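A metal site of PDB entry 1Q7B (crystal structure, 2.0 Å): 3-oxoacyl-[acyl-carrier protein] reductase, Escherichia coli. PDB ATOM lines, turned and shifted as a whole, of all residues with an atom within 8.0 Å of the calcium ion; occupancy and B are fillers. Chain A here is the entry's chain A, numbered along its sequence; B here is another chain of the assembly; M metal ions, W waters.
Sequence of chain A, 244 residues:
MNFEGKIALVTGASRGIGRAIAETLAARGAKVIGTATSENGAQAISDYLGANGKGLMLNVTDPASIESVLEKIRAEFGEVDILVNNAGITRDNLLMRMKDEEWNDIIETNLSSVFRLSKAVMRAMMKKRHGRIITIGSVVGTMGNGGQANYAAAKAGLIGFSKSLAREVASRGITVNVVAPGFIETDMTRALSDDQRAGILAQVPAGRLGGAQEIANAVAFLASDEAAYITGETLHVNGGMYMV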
ATOM      1  N   VAL A 178      24.554 -17.364  12.999  1.00  0.00           N
ATOM      2  CA  VAL A 178      25.365 -16.851  11.915  1.00  0.00           C
ATOM      3  C   VAL A 178      25.096 -17.648  10.636  1.00  0.00           C
ATOM      4  O   VAL A 178      24.973 -18.873  10.675  1.00  0.00           O
ATOM      5  CB  VAL A 178      26.875 -16.960  12.239  1.00  0.00           C
ATOM      6  CG1 VAL A 178      27.710 -16.510  11.044  1.00  0.00           C
ATOM      7  CG2 VAL A 178      27.209 -16.132  13.474  1.00  0.00           C
ATOM      8  N   GLY A 232      23.372 -20.057  18.632  1.00  0.00           N
ATOM      9  CA  GLY A 232      24.804 -20.220  18.790  1.00  0.00           C
ATOM     10  C   GLY A 232      25.325 -21.089  17.655  1.00  0.00           C
ATOM     11  O   GLY A 232      26.448 -21.608  17.719  1.00  0.00           O
ATOM     12  N   GLU A 233      24.508 -21.221  16.618  1.00  0.00           N
ATOM     13  CA  GLU A 233      24.844 -22.052  15.458  1.00  0.00           C
ATOM     14  C   GLU A 233      25.269 -21.273  14.216  1.00  0.00           C
ATOM     15  O   GLU A 233      24.862 -20.127  13.999  1.00  0.00           O
ATOM     16  CB  GLU A 233      23.654 -22.963  15.119  1.00  0.00           C
ATOM     17  CG  GLU A 233      23.668 -23.607  13.722  1.00  0.00           C
ATOM     18  CD  GLU A 233      24.707 -24.710  13.564  1.00  0.00           C
ATOM     19  OE1 GLU A 233      25.700 -24.727  14.319  1.00  0.00           O
ATOM     20  OE2 GLU A 233      24.535 -25.560  12.658  1.00  0.00           O
ATOM     21  N   THR A 234      26.129 -21.904  13.415  1.00  0.00           N
ATOM     22  CA  THR A 234      26.607 -21.316  12.167  1.00  0.00           C
ATOM     23  C   THR A 234      26.077 -22.179  11.026  1.00  0.00           C
ATOM     24  O   THR A 234      26.400 -23.376  10.952  1.00  0.00           O
ATOM     25  CB  THR A 234      28.145 -21.296  12.081  1.00  0.00           C
ATOM     26  OG1 THR A 234      28.687 -20.490  13.119  1.00  0.00           O
ATOM     27  CG2 THR A 234      28.592 -20.718  10.732  1.00  0.00           C
ATOM     28  N   LEU A 235      25.254 -21.599  10.163  1.00  0.00           N
ATOM     29  CA  LEU A 235      24.696 -22.323   9.041  1.00  0.00           C
ATOM     30  C   LEU A 235      25.500 -21.984   7.793  1.00  0.00           C
ATOM     31  O   LEU A 235      25.424 -20.853   7.286  1.00  0.00           O
ATOM     32  CB  LEU A 235      23.217 -21.953   8.850  1.00  0.00           C
ATOM     33  CG  LEU A 235      22.507 -22.501   7.605  1.00  0.00           C
ATOM     34  CD1 LEU A 235      22.614 -24.018   7.535  1.00  0.00           C
ATOM     35  CD2 LEU A 235      21.054 -22.060   7.640  1.00  0.00           C
ATOM     36  N   HIS A 236      26.285 -22.943   7.298  1.00  0.00           N
ATOM     37  CA  HIS A 236      27.099 -22.725   6.109  1.00  0.00           C
ATOM     38  C   HIS A 236      26.321 -22.926   4.821  1.00  0.00           C
ATOM     39  O   HIS A 236      25.671 -23.953   4.622  1.00  0.00           O
ATOM     40  CB  HIS A 236      28.315 -23.659   6.137  1.00  0.00           C
ATOM     41  CG  HIS A 236      29.287 -23.345   7.231  1.00  0.00           C
ATOM     42  ND1 HIS A 236      29.265 -23.996   8.446  1.00  0.00           N
ATOM     43  CD2 HIS A 236      30.280 -22.427   7.305  1.00  0.00           C
ATOM     44  CE1 HIS A 236      30.198 -23.487   9.230  1.00  0.00           C
ATOM     45  NE2 HIS A 236      30.824 -22.531   8.562  1.00  0.00           N
ATOM     46  N   VAL A 244      32.244 -28.496   7.421  1.00  0.00           N
ATOM     47  CA  VAL A 244      32.560 -28.708   8.823  1.00  0.00           C
ATOM     48  C   VAL A 244      31.357 -29.327   9.525  1.00  0.00           C
ATOM     49  O   VAL A 244      31.568 -30.263  10.322  1.00  0.00           O
ATOM     50  CB  VAL A 244      32.990 -27.384   9.526  1.00  0.00           C
ATOM     51  CG1 VAL A 244      34.309 -26.886   8.940  1.00  0.00           C
ATOM     52  CG2 VAL A 244      31.907 -26.315   9.372  1.00  0.00           C
ATOM     53  OXT VAL A 244      30.221 -28.882   9.269  1.00  0.00           O
ATOM     54  N   VAL B 178      23.077 -32.995   7.146  1.00  0.00           N
ATOM     55  CA  VAL B 178      22.762 -33.620   8.413  1.00  0.00           C
ATOM     56  C   VAL B 178      22.118 -32.613   9.357  1.00  0.00           C
ATOM     57  O   VAL B 178      22.561 -31.461   9.437  1.00  0.00           O
ATOM     58  CB  VAL B 178      24.046 -34.170   9.104  1.00  0.00           C
ATOM     59  CG1 VAL B 178      23.720 -34.751  10.483  1.00  0.00           C
ATOM     60  CG2 VAL B 178      24.698 -35.225   8.211  1.00  0.00           C
ATOM     61  N   GLY B 232      26.818 -30.850   2.443  1.00  0.00           N
ATOM     62  CA  GLY B 232      27.951 -31.290   3.246  1.00  0.00           C
ATOM     63  C   GLY B 232      27.948 -30.557   4.567  1.00  0.00           C
ATOM     64  O   GLY B 232      28.953 -30.529   5.286  1.00  0.00           O
ATOM     65  N   GLU B 233      26.800 -29.984   4.912  1.00  0.00           N
ATOM     66  CA  GLU B 233      26.654 -29.189   6.138  1.00  0.00           C
ATOM     67  C   GLU B 233      25.869 -29.892   7.231  1.00  0.00           C
ATOM     68  O   GLU B 233      25.006 -30.743   6.966  1.00  0.00           O
ATOM     69  CB  GLU B 233      25.992 -27.844   5.793  1.00  0.00           C
ATOM     70  CG  GLU B 233      25.386 -27.077   6.984  1.00  0.00           C
ATOM     71  CD  GLU B 233      26.437 -26.461   7.895  1.00  0.00           C
ATOM     72  OE1 GLU B 233      27.579 -26.961   7.924  1.00  0.00           O
ATOM     73  OE2 GLU B 233      26.094 -25.482   8.585  1.00  0.00           O
ATOM     74  N   THR B 234      26.196 -29.549   8.474  1.00  0.00           N
ATOM     75  CA  THR B 234      25.514 -30.091   9.641  1.00  0.00           C
ATOM     76  C   THR B 234      24.784 -28.930  10.323  1.00  0.00           C
ATOM     77  O   THR B 234      25.412 -27.969  10.761  1.00  0.00           O
ATOM     78  CB  THR B 234      26.509 -30.702  10.660  1.00  0.00           C
ATOM     79  OG1 THR B 234      27.214 -31.781  10.047  1.00  0.00           O
ATOM     80  CG2 THR B 234      25.762 -31.209  11.895  1.00  0.00           C
ATOM     81  N   LEU B 235      23.465 -29.024  10.400  1.00  0.00           N
ATOM     82  CA  LEU B 235      22.672 -27.983  11.041  1.00  0.00           C
ATOM     83  C   LEU B 235      22.330 -28.436  12.462  1.00  0.00           C
ATOM     84  O   LEU B 235      21.542 -29.366  12.657  1.00  0.00           O
ATOM     85  CB  LEU B 235      21.391 -27.728  10.244  1.00  0.00           C
ATOM     86  CG  LEU B 235      20.356 -26.767  10.851  1.00  0.00           C
ATOM     87  CD1 LEU B 235      21.006 -25.415  11.177  1.00  0.00           C
ATOM     88  CD2 LEU B 235      19.216 -26.590   9.859  1.00  0.00           C
ATOM     89  N   HIS B 236      22.937 -27.797  13.458  1.00  0.00           N
ATOM     90  CA  HIS B 236      22.679 -28.163  14.843  1.00  0.00           C
ATOM     91  C   HIS B 236      21.427 -27.488  15.393  1.00  0.00           C
ATOM     92  O   HIS B 236      21.266 -26.281  15.302  1.00  0.00           O
ATOM     93  CB  HIS B 236      23.884 -27.799  15.720  1.00  0.00           C
ATOM     94  CG  HIS B 236      25.096 -28.625  15.421  1.00  0.00           C
ATOM     95  ND1 HIS B 236      26.090 -28.197  14.565  1.00  0.00           N
ATOM     96  CD2 HIS B 236      25.451 -29.868  15.818  1.00  0.00           C
ATOM     97  CE1 HIS B 236      27.005 -29.135  14.445  1.00  0.00           C
ATOM     98  NE2 HIS B 236      26.640 -30.159  15.196  1.00  0.00           N
ATOM     99  N   VAL B 244      29.259 -25.029  17.823  1.00  0.00           N
ATOM    100  CA  VAL B 244      30.433 -25.131  16.979  1.00  0.00           C
ATOM    101  C   VAL B 244      30.276 -24.221  15.772  1.00  0.00           C
ATOM    102  O   VAL B 244      31.281 -23.574  15.392  1.00  0.00           O
ATOM    103  CB  VAL B 244      30.668 -26.580  16.521  1.00  0.00           C
ATOM    104  CG1 VAL B 244      30.990 -27.468  17.740  1.00  0.00           C
ATOM    105  CG2 VAL B 244      29.448 -27.090  15.799  1.00  0.00           C
ATOM    106  OXT VAL B 244      29.160 -24.158  15.205  1.00  0.00           O
HETATM  107 CA    CA M   1      26.366 -25.740  11.005  1.00  0.00          CA
HETATM  108  O   HOH W   1      27.931 -25.529  12.823  1.00  0.00           O
HETATM  109  O   HOH W   2      28.437 -26.855  10.498  1.00  0.00           O
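The side-chain carboxylate of Glu 233 of chain B sits at hydrogen-bond distance from a ring nitrogen (ND1) of His 236 of chain A, 3.5 Å away.
The backbone carbonyl oxygen of Glu 233 of chain B lies within hydrogen-bond range of the backbone NH of Val 178 of chain B (3.0 Å).
OE2 of Glu 233 of chain A sits close to N of His 236 of chain B, 2.9 Å away.
O of Glu 233 of chain A is in hydrogen-bond range of N of Val 178 of chain A (3.0 Å).
Within 4 Å of the calcium ion: Glu 233 of chain A, Thr 234 of chain A, Glu 233 of chain B and Thr 234 of chain B.
The calcium ion is bound by the backbone carbonyl oxygen of Thr 234 of chain A (2.4 Å), water W2 (2.4 Å), water W1 (2.4 Å), the backbone carbonyl oxygen of Thr 234 of chain B (2.4 Å), the side-chain carboxylate of Glu 233 of chain B (2.4 Å) and the side-chain carboxylate of Glu 233 of chain A (2.5 Å).
The calcium ion has six donor atoms within binding distance.
Water W1 lies within hydrogen-bond range of OE1 of Glu 233 of chain A (2.8 Å) and OXT of Val 244 of chain B (3.0 Å).
Water W2 lies within hydrogen-bond range of the side-chain carboxylate of Glu 233 of chain B and the chain-end carboxylate of Val 244 of chain A.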
